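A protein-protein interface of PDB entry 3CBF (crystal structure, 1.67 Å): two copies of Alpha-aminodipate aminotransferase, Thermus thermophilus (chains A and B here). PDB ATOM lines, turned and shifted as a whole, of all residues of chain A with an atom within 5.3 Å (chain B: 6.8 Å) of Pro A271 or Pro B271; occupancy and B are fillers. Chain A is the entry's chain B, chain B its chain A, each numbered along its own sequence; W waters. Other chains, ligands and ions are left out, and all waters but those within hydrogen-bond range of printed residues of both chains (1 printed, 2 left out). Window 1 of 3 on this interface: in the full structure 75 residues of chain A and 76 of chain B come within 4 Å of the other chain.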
ATOM      1  N   THR A  98      -0.982  -7.665   0.304  1.00  0.00           N
ATOM      2  CA  THR A  98      -1.211  -6.474   1.122  1.00  0.00           C
ATOM      3  C   THR A  98      -1.249  -6.878   2.608  1.00  0.00           C
ATOM      4  O   THR A  98      -2.336  -6.980   3.250  1.00  0.00           O
ATOM      5  CB  THR A  98      -2.506  -5.760   0.651  1.00  0.00           C
ATOM      6  OG1 THR A  98      -2.448  -5.516  -0.765  1.00  0.00           O
ATOM      7  CG2 THR A  98      -2.723  -4.441   1.382  1.00  0.00           C
ATOM      8  N   GLY A 243       2.818  -0.685   8.611  1.00  0.00           N
ATOM      9  CA  GLY A 243       1.925   0.288   7.984  1.00  0.00           C
ATOM     10  C   GLY A 243       1.972   0.282   6.467  1.00  0.00           C
ATOM     11  O   GLY A 243       0.987   0.689   5.812  1.00  0.00           O
ATOM     12  N   LEU A 244       3.087  -0.195   5.894  1.00  0.00           N
ATOM     13  CA  LEU A 244       3.202  -0.234   4.438  1.00  0.00           C
ATOM     14  C   LEU A 244       2.307  -1.324   3.796  1.00  0.00           C
ATOM     15  O   LEU A 244       2.006  -1.283   2.596  1.00  0.00           O
ATOM     16  CB  LEU A 244       4.668  -0.402   3.974  1.00  0.00           C
ATOM     17  CG  LEU A 244       5.601   0.815   4.118  1.00  0.00           C
ATOM     18  CD1 LEU A 244       6.967   0.442   3.623  1.00  0.00           C
ATOM     19  CD2 LEU A 244       5.076   2.033   3.325  1.00  0.00           C
ATOM     20  N   ARG A 245       1.900  -2.287   4.628  1.00  0.00           N
ATOM     21  CA  ARG A 245       1.168  -3.490   4.207  1.00  0.00           C
ATOM     22  C   ARG A 245       1.776  -4.208   3.007  1.00  0.00           C
ATOM     23  O   ARG A 245       1.200  -4.178   1.907  1.00  0.00           O
ATOM     24  CB  ARG A 245      -0.302  -3.174   3.891  1.00  0.00           C
ATOM     25  CG  ARG A 245      -1.020  -2.177   4.807  1.00  0.00           C
ATOM     26  CD  ARG A 245      -1.213  -2.589   6.255  1.00  0.00           C
ATOM     27  NE  ARG A 245      -1.839  -3.918   6.386  1.00  0.00           N
ATOM     28  CZ  ARG A 245      -1.231  -4.996   6.910  1.00  0.00           C
ATOM     29  NH1 ARG A 245       0.019  -4.945   7.338  1.00  0.00           N
ATOM     30  NH2 ARG A 245      -1.908  -6.159   7.014  1.00  0.00           N
ATOM     31  N   HIS A 269      -4.306  -5.167  -6.883  1.00  0.00           N
ATOM     32  CA  HIS A 269      -2.900  -5.342  -6.577  1.00  0.00           C
ATOM     33  C   HIS A 269      -2.534  -4.532  -5.313  1.00  0.00           C
ATOM     34  O   HIS A 269      -3.194  -3.547  -4.949  1.00  0.00           O
ATOM     35  CB  HIS A 269      -2.021  -4.926  -7.793  1.00  0.00           C
ATOM     36  CG  HIS A 269      -1.972  -3.446  -8.062  1.00  0.00           C
ATOM     37  ND1 HIS A 269      -2.804  -2.802  -8.962  1.00  0.00           N
ATOM     38  CD2 HIS A 269      -1.153  -2.488  -7.568  1.00  0.00           C
ATOM     39  CE1 HIS A 269      -2.498  -1.513  -9.005  1.00  0.00           C
ATOM     40  NE2 HIS A 269      -1.515  -1.300  -8.155  1.00  0.00           N
ATOM     41  N   THR A 270      -1.510  -5.006  -4.627  1.00  0.00           N
ATOM     42  CA  THR A 270      -0.820  -4.228  -3.592  1.00  0.00           C
ATOM     43  C   THR A 270      -0.236  -2.913  -4.165  1.00  0.00           C
ATOM     44  O   THR A 270       0.352  -2.914  -5.250  1.00  0.00           O
ATOM     45  CB  THR A 270       0.291  -5.095  -2.960  1.00  0.00           C
ATOM     46  OG1 THR A 270      -0.288  -6.302  -2.441  1.00  0.00           O
ATOM     47  CG2 THR A 270       1.019  -4.386  -1.818  1.00  0.00           C
ATOM     48  N   PRO A 271      -0.425  -1.810  -3.441  1.00  0.00           N
ATOM     49  CA  PRO A 271       0.096  -0.539  -3.993  1.00  0.00           C
ATOM     50  C   PRO A 271       1.551  -0.623  -4.383  1.00  0.00           C
ATOM     51  O   PRO A 271       2.395  -1.161  -3.630  1.00  0.00           O
ATOM     52  CB  PRO A 271      -0.114   0.475  -2.883  1.00  0.00           C
ATOM     53  CG  PRO A 271      -0.548  -0.259  -1.681  1.00  0.00           C
ATOM     54  CD  PRO A 271      -1.092  -1.623  -2.140  1.00  0.00           C
ATOM     55  N   MET A 272       1.860  -0.024  -5.535  1.00  0.00           N
ATOM     56  CA  MET A 272       3.166  -0.121  -6.143  1.00  0.00           C
ATOM     57  C   MET A 272       4.238   0.662  -5.395  1.00  0.00           C
ATOM     58  O   MET A 272       5.335   0.163  -5.172  1.00  0.00           O
ATOM     59  CB  MET A 272       3.092   0.358  -7.595  1.00  0.00           C
ATOM     60  CG  MET A 272       4.080  -0.327  -8.460  1.00  0.00           C
ATOM     61  SD  MET A 272       3.730  -2.079  -8.481  1.00  0.00           S
ATOM     62  CE  MET A 272       4.906  -2.591  -9.730  1.00  0.00           C
ATOM     63  N   LEU A 273       3.903   1.909  -5.026  1.00  0.00           N
ATOM     64  CA  LEU A 273       4.805   2.737  -4.225  1.00  0.00           C
ATOM     65  C   LEU A 273       5.390   1.968  -3.026  1.00  0.00           C
ATOM     66  O   LEU A 273       6.605   2.013  -2.772  1.00  0.00           O
ATOM     67  CB  LEU A 273       4.103   4.011  -3.761  1.00  0.00           C
ATOM     68  CG  LEU A 273       4.821   4.924  -2.750  1.00  0.00           C
ATOM     69  CD1 LEU A 273       6.191   5.450  -3.275  1.00  0.00           C
ATOM     70  CD2 LEU A 273       3.898   6.079  -2.404  1.00  0.00           C
ATOM     71  N   ASN A 274       4.508   1.234  -2.332  1.00  0.00           N
ATOM     72  CA  ASN A 274       4.850   0.552  -1.088  1.00  0.00           C
ATOM     73  C   ASN A 274       5.809  -0.602  -1.371  1.00  0.00           C
ATOM     74  O   ASN A 274       6.814  -0.773  -0.654  1.00  0.00           O
ATOM     75  CB  ASN A 274       3.578   0.025  -0.413  1.00  0.00           C
ATOM     76  CG  ASN A 274       2.570   1.109  -0.114  1.00  0.00           C
ATOM     77  OD1 ASN A 274       2.059   1.195   1.009  1.00  0.00           O
ATOM     78  ND2 ASN A 274       2.243   1.903  -1.102  1.00  0.00           N
ATOM     79  N   GLN A 275       5.529  -1.348  -2.453  1.00  0.00           N
ATOM     80  CA  GLN A 275       6.403  -2.446  -2.879  1.00  0.00           C
ATOM     81  C   GLN A 275       7.779  -1.945  -3.277  1.00  0.00           C
ATOM     82  O   GLN A 275       8.793  -2.534  -2.898  1.00  0.00           O
ATOM     83  CB  GLN A 275       5.804  -3.146  -4.081  1.00  0.00           C
ATOM     84  CG  GLN A 275       4.507  -3.815  -3.759  1.00  0.00           C
ATOM     85  CD  GLN A 275       4.021  -4.653  -4.919  1.00  0.00           C
ATOM     86  OE1 GLN A 275       4.695  -5.592  -5.366  1.00  0.00           O
ATOM     87  NE2 GLN A 275       2.859  -4.300  -5.428  1.00  0.00           N
ATOM     88  N   ALA B  67       2.721   6.835   9.869  1.00  0.00           N
ATOM     89  CA  ALA B  67       2.600   6.315   8.507  1.00  0.00           C
ATOM     90  C   ALA B  67       3.078   4.879   8.368  1.00  0.00           C
ATOM     91  O   ALA B  67       2.558   4.122   7.527  1.00  0.00           O
ATOM     92  CB  ALA B  67       3.349   7.189   7.522  1.00  0.00           C
ATOM     93  N   ILE B  96     -12.336   3.910   4.743  1.00  0.00           N
ATOM     94  CA  ILE B  96     -11.275   3.892   3.734  1.00  0.00           C
ATOM     95  C   ILE B  96     -10.922   2.439   3.351  1.00  0.00           C
ATOM     96  O   ILE B  96     -10.625   1.619   4.220  1.00  0.00           O
ATOM     97  CB  ILE B  96      -9.985   4.668   4.189  1.00  0.00           C
ATOM     98  CG1 ILE B  96     -10.336   6.088   4.689  1.00  0.00           C
ATOM     99  CG2 ILE B  96      -8.949   4.753   3.038  1.00  0.00           C
ATOM    100  CD1 ILE B  96     -11.210   6.892   3.702  1.00  0.00           C
ATOM    101  N   THR B  98      -8.987  -0.365   0.276  1.00  0.00           N
ATOM    102  CA  THR B  98      -7.756  -0.549  -0.512  1.00  0.00           C
ATOM    103  C   THR B  98      -8.171  -0.637  -1.982  1.00  0.00           C
ATOM    104  O   THR B  98      -8.136  -1.711  -2.611  1.00  0.00           O
ATOM    105  CB  THR B  98      -6.960  -1.777  -0.006  1.00  0.00           C
ATOM    106  OG1 THR B  98      -6.679  -1.601   1.383  1.00  0.00           O
ATOM    107  CG2 THR B  98      -5.631  -1.939  -0.753  1.00  0.00           C
ATOM    108  N   PRO B 242      -4.378   5.479  -9.341  1.00  0.00           N
ATOM    109  CA  PRO B 242      -4.888   4.126  -9.130  1.00  0.00           C
ATOM    110  C   PRO B 242      -3.881   3.279  -8.341  1.00  0.00           C
ATOM    111  O   PRO B 242      -4.266   2.479  -7.493  1.00  0.00           O
ATOM    112  CB  PRO B 242      -5.078   3.583 -10.559  1.00  0.00           C
ATOM    113  CG  PRO B 242      -4.307   4.448 -11.427  1.00  0.00           C
ATOM    114  CD  PRO B 242      -4.092   5.752 -10.759  1.00  0.00           C
ATOM    115  N   GLY B 243      -2.593   3.498  -8.587  1.00  0.00           N
ATOM    116  CA  GLY B 243      -1.538   2.708  -7.944  1.00  0.00           C
ATOM    117  C   GLY B 243      -1.448   2.833  -6.437  1.00  0.00           C
ATOM    118  O   GLY B 243      -0.907   1.950  -5.759  1.00  0.00           O
ATOM    119  N   LEU B 244      -2.004   3.916  -5.898  1.00  0.00           N
ATOM    120  CA  LEU B 244      -1.965   4.129  -4.467  1.00  0.00           C
ATOM    121  C   LEU B 244      -2.941   3.225  -3.724  1.00  0.00           C
ATOM    122  O   LEU B 244      -2.740   2.981  -2.543  1.00  0.00           O
ATOM    123  CB  LEU B 244      -2.186   5.610  -4.101  1.00  0.00           C
ATOM    124  CG  LEU B 244      -1.015   6.602  -4.333  1.00  0.00           C
ATOM    125  CD1 LEU B 244      -1.399   7.945  -3.764  1.00  0.00           C
ATOM    126  CD2 LEU B 244       0.305   6.120  -3.698  1.00  0.00           C
ATOM    127  N   ARG B 245      -4.007   2.795  -4.419  1.00  0.00           N
ATOM    128  CA  ARG B 245      -5.021   1.861  -3.876  1.00  0.00           C
ATOM    129  C   ARG B 245      -5.748   2.483  -2.674  1.00  0.00           C
ATOM    130  O   ARG B 245      -5.654   1.966  -1.553  1.00  0.00           O
ATOM    131  CB  ARG B 245      -4.382   0.538  -3.466  1.00  0.00           C
ATOM    132  CG  ARG B 245      -3.452  -0.154  -4.478  1.00  0.00           C
ATOM    133  CD  ARG B 245      -4.075  -0.478  -5.863  1.00  0.00           C
ATOM    134  NE  ARG B 245      -5.371  -1.198  -5.817  1.00  0.00           N
ATOM    135  CZ  ARG B 245      -6.517  -0.737  -6.343  1.00  0.00           C
ATOM    136  NH1 ARG B 245      -6.599   0.453  -6.943  1.00  0.00           N
ATOM    137  NH2 ARG B 245      -7.614  -1.467  -6.276  1.00  0.00           N
ATOM    138  N   VAL B 246      -6.418   3.619  -2.896  1.00  0.00           N
ATOM    139  CA  VAL B 246      -7.138   4.320  -1.809  1.00  0.00           C
ATOM    140  C   VAL B 246      -8.497   4.722  -2.293  1.00  0.00           C
ATOM    141  O   VAL B 246      -8.628   5.398  -3.325  1.00  0.00           O
ATOM    142  CB  VAL B 246      -6.332   5.582  -1.281  1.00  0.00           C
ATOM    143  CG1 VAL B 246      -7.105   6.333  -0.220  1.00  0.00           C
ATOM    144  CG2 VAL B 246      -4.930   5.167  -0.750  1.00  0.00           C
ATOM    145  N   LYS B 263     -13.244  -6.111   6.649  1.00  0.00           N
ATOM    146  CA  LYS B 263     -11.942  -5.555   6.237  1.00  0.00           C
ATOM    147  C   LYS B 263     -10.796  -5.939   7.189  1.00  0.00           C
ATOM    148  O   LYS B 263      -9.639  -6.117   6.765  1.00  0.00           O
ATOM    149  CB  LYS B 263     -12.011  -4.049   6.075  1.00  0.00           C
ATOM    150  CG  LYS B 263     -10.661  -3.419   5.734  1.00  0.00           C
ATOM    151  CD  LYS B 263     -10.832  -2.050   5.108  1.00  0.00           C
ATOM    152  CE  LYS B 263      -9.518  -1.283   5.134  1.00  0.00           C
ATOM    153  NZ  LYS B 263      -8.496  -1.885   4.191  1.00  0.00           N
ATOM    154  N   ASP B 267      -7.321  -7.349   5.235  1.00  0.00           N
ATOM    155  CA  ASP B 267      -5.961  -6.694   5.151  1.00  0.00           C
ATOM    156  C   ASP B 267      -5.517  -5.872   6.378  1.00  0.00           C
ATOM    157  O   ASP B 267      -4.525  -5.129   6.327  1.00  0.00           O
ATOM    158  CB  ASP B 267      -5.835  -5.882   3.840  1.00  0.00           C
ATOM    159  CG  ASP B 267      -6.727  -4.620   3.802  1.00  0.00           C
ATOM    160  OD1 ASP B 267      -6.846  -4.012   2.698  1.00  0.00           O
ATOM    161  OD2 ASP B 267      -7.278  -4.241   4.856  1.00  0.00           O
ATOM    162  N   HIS B 269      -5.795  -3.035   7.565  1.00  0.00           N
ATOM    163  CA  HIS B 269      -6.082  -1.654   7.233  1.00  0.00           C
ATOM    164  C   HIS B 269      -5.366  -1.306   5.925  1.00  0.00           C
ATOM    165  O   HIS B 269      -4.346  -1.926   5.569  1.00  0.00           O
ATOM    166  CB  HIS B 269      -5.661  -0.706   8.371  1.00  0.00           C
ATOM    167  CG  HIS B 269      -4.181  -0.533   8.530  1.00  0.00           C
ATOM    168  ND1 HIS B 269      -3.415  -1.308   9.379  1.00  0.00           N
ATOM    169  CD2 HIS B 269      -3.336   0.374   7.985  1.00  0.00           C
ATOM    170  CE1 HIS B 269      -2.152  -0.907   9.317  1.00  0.00           C
ATOM    171  NE2 HIS B 269      -2.081   0.118   8.490  1.00  0.00           N
ATOM    172  N   THR B 270      -5.948  -0.346   5.212  1.00  0.00           N
ATOM    173  CA  THR B 270      -5.313   0.261   4.032  1.00  0.00           C
ATOM    174  C   THR B 270      -4.006   0.930   4.460  1.00  0.00           C
ATOM    175  O   THR B 270      -3.965   1.559   5.500  1.00  0.00           O
ATOM    176  CB  THR B 270      -6.314   1.269   3.401  1.00  0.00           C
ATOM    177  OG1 THR B 270      -7.510   0.549   3.024  1.00  0.00           O
ATOM    178  CG2 THR B 270      -5.770   1.960   2.148  1.00  0.00           C
ATOM    179  N   PRO B 271      -2.919   0.778   3.659  1.00  0.00           N
ATOM    180  CA  PRO B 271      -1.660   1.381   4.121  1.00  0.00           C
ATOM    181  C   PRO B 271      -1.761   2.859   4.422  1.00  0.00           C
ATOM    182  O   PRO B 271      -2.391   3.625   3.686  1.00  0.00           O
ATOM    183  CB  PRO B 271      -0.700   1.145   2.967  1.00  0.00           C
ATOM    184  CG  PRO B 271      -1.522   0.870   1.832  1.00  0.00           C
ATOM    185  CD  PRO B 271      -2.723   0.085   2.388  1.00  0.00           C
ATOM    186  N   MET B 272      -1.111   3.237   5.508  1.00  0.00           N
ATOM    187  CA  MET B 272      -1.284   4.536   6.086  1.00  0.00           C
ATOM    188  C   MET B 272      -0.604   5.658   5.271  1.00  0.00           C
ATOM    189  O   MET B 272      -1.184   6.714   5.073  1.00  0.00           O
ATOM    190  CB  MET B 272      -0.745   4.503   7.498  1.00  0.00           C
ATOM    191  CG  MET B 272      -1.359   5.504   8.378  1.00  0.00           C
ATOM    192  SD  MET B 272      -3.158   5.376   8.499  1.00  0.00           S
ATOM    193  CE  MET B 272      -3.395   6.468   9.893  1.00  0.00           C
ATOM    194  N   LEU B 273       0.612   5.410   4.809  1.00  0.00           N
ATOM    195  CA  LEU B 273       1.320   6.383   3.968  1.00  0.00           C
ATOM    196  C   LEU B 273       0.396   6.817   2.829  1.00  0.00           C
ATOM    197  O   LEU B 273       0.243   8.013   2.543  1.00  0.00           O
ATOM    198  CB  LEU B 273       2.598   5.735   3.404  1.00  0.00           C
ATOM    199  CG  LEU B 273       3.384   6.512   2.341  1.00  0.00           C
ATOM    200  CD1 LEU B 273       3.746   7.941   2.854  1.00  0.00           C
ATOM    201  CD2 LEU B 273       4.605   5.703   2.016  1.00  0.00           C
ATOM    202  N   ASN B 274      -0.242   5.832   2.205  1.00  0.00           N
ATOM    203  CA  ASN B 274      -1.047   6.055   1.015  1.00  0.00           C
ATOM    204  C   ASN B 274      -2.231   7.001   1.320  1.00  0.00           C
ATOM    205  O   ASN B 274      -2.538   7.920   0.547  1.00  0.00           O
ATOM    206  CB  ASN B 274      -1.484   4.698   0.445  1.00  0.00           C
ATOM    207  CG  ASN B 274      -0.294   3.808   0.107  1.00  0.00           C
ATOM    208  OD1 ASN B 274      -0.139   3.354  -1.033  1.00  0.00           O
ATOM    209  ND2 ASN B 274       0.553   3.566   1.095  1.00  0.00           N
ATOM    210  N   GLN B 275      -2.886   6.778   2.462  1.00  0.00           N
ATOM    211  CA  GLN B 275      -4.026   7.605   2.861  1.00  0.00           C
ATOM    212  C   GLN B 275      -3.603   9.029   3.166  1.00  0.00           C
ATOM    213  O   GLN B 275      -4.244   9.975   2.741  1.00  0.00           O
ATOM    214  CB  GLN B 275      -4.730   7.001   4.085  1.00  0.00           C
ATOM    215  CG  GLN B 275      -5.280   5.597   3.897  1.00  0.00           C
ATOM    216  CD  GLN B 275      -6.029   5.158   5.141  1.00  0.00           C
ATOM    217  OE1 GLN B 275      -6.977   5.819   5.560  1.00  0.00           O
ATOM    218  NE2 GLN B 275      -5.594   4.042   5.756  1.00  0.00           N
ATOM    219  N   MET B 276      -2.512   9.163   3.916  1.00  0.00           N
ATOM    220  CA  MET B 276      -1.954  10.468   4.273  1.00  0.00           C
ATOM    221  C   MET B 276      -1.505  11.236   3.013  1.00  0.00           C
ATOM    222  O   MET B 276      -1.702  12.450   2.897  1.00  0.00           O
ATOM    223  CB  MET B 276      -0.792  10.240   5.240  1.00  0.00           C
ATOM    224  CG  MET B 276      -1.266   9.705   6.590  1.00  0.00           C
ATOM    225  SD  MET B 276       0.052   9.089   7.629  1.00  0.00           S
ATOM    226  CE  MET B 276       0.636  10.672   8.216  1.00  0.00           C
HETATM  227  O   HOH W   1       1.358   3.074  -5.325  1.00  0.00           O
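The side-chain carboxylate (OD1) of Asp B267 is in hydrogen-bond range of the side-chain hydroxyl (OG1) of Thr B98, 2.8 Å away.
O of Pro B242 sits at hydrogen-bond distance from NH1 of Arg B245 (3.1 Å).
The side-chain amide oxygen (OD1) of Asn B274 sits close to the backbone carbonyl oxygen (O) of Leu B244 (3.0 Å).
OD2 of Asp B267 lies close to N of His B269 (3.3 Å).
OG1 of Thr A98 is in hydrogen-bond range of OG1 of Thr A270 (2.8 Å).
The side-chain amide oxygen of Asn A274 sits close to the backbone carbonyl oxygen of Leu A244.
Thr A98 touches Asp B267.
CA of Gly A243 touches O of Ala B67, at 3.9 Å.
Gly A243 touches Pro B271 (O to CA, 3.2 Å).
Leu B273 touches Leu A244 (CD2 to CD2, 3.9 Å).
O of Gly B243 touches CA of Pro A271, 3.2 Å away.
Pro A271 touches Leu B244 (CB to O, 3.6 Å).
CA of Pro A271 touches CG of Arg B245 (3.6 Å).
Pro A271 touches Pro B271 (CG to CG, 3.8 Å).
Pro A271 touches Asn B274 (CB to OD1, 3.4 Å).
Leu A273 touches Leu B244.
Gly A243 touches Pro B271, and with the chains exchanged Pro A271 touches Gly B243.
Leu A244 touches Leu B273, and with the chains exchanged Leu A273 touches Leu B244.
Arg A245 touches Pro B271, and with the chains exchanged Pro A271 touches Arg B245.
Asn A274 touches its own counterpart, Asn B274.
Positions printed for both chains: 98, 243, 244, 245, 269, 270, 271, 272, 273, 274 and 275.
Of the printed residues of chain B, Arg A245 touches Asp B267, His B269 and Pro B271.
Pro A271 touches just these residues of chain B: Gly B243, Leu B244, Arg B245, Pro B271 and Asn B274.
Of the printed residues of chain B, Met A272 touches Gly B243.
Of the printed residues of chain A, Ala B67 touches Gly A243 (3.9 Å).
Thr B98 touches none of the printed residues of chain A.
Pro B242 touches none of the printed residues of chain A.
Of the printed residues of chain A, Arg B245 touches His A269 (3.3 Å) and Pro A271 (3.6 Å).
Printed residues of chain A within 4 Å of His B269: Arg A245.
Of chain A, only Gly A243 (3.2 Å), Leu A244 (3.7 Å), Arg A245 (3.7 Å), Pro A271 (3.8 Å) and Asn A274 (3.4 Å) come within 4 Å of Pro B271.
The nearest residue of chain A that does not touch Pro B271 is Thr A98 (4.6 Å).
The backbone NH (N) of Met A272 sits at hydrogen-bond distance from the backbone carbonyl oxygen (O) of Gly B243, 3.4 Å away.
The guanidinium group (NE) of Arg B245 is in hydrogen-bond range of the backbone carbonyl oxygen (O) of His A269 (3.3 Å).
The backbone carbonyl oxygen (O) of Asp B267 lies within hydrogen-bond range of the guanidinium group (NH2) of Arg A245 (2.9 Å).
O of His B269 lies close to NE of Arg A245 (3.3 Å).
N of Met B272 lies within hydrogen-bond range of O of Gly A243.
The side-chain amide oxygen of Asn B274 sits at hydrogen-bond distance from the side-chain amide nitrogen of Asn A274 (2.8 Å).
Printed residues of chain A that touch a printed residue of chain B: Thr A98, Gly A243, Leu A244, Arg A245, His A269, Pro A271, Met A272, Leu A273 and Asn A274.
Among the printed residues, no Asp or Glu carboxylate lies within 4 Å of a Lys or Arg side-chain nitrogen of the other chain.
Water W1 lies within hydrogen-bond range of O of Gly B243 (2.6 Å), N of Leu A273 (2.8 Å) and N of Met A272 (3.1 Å).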
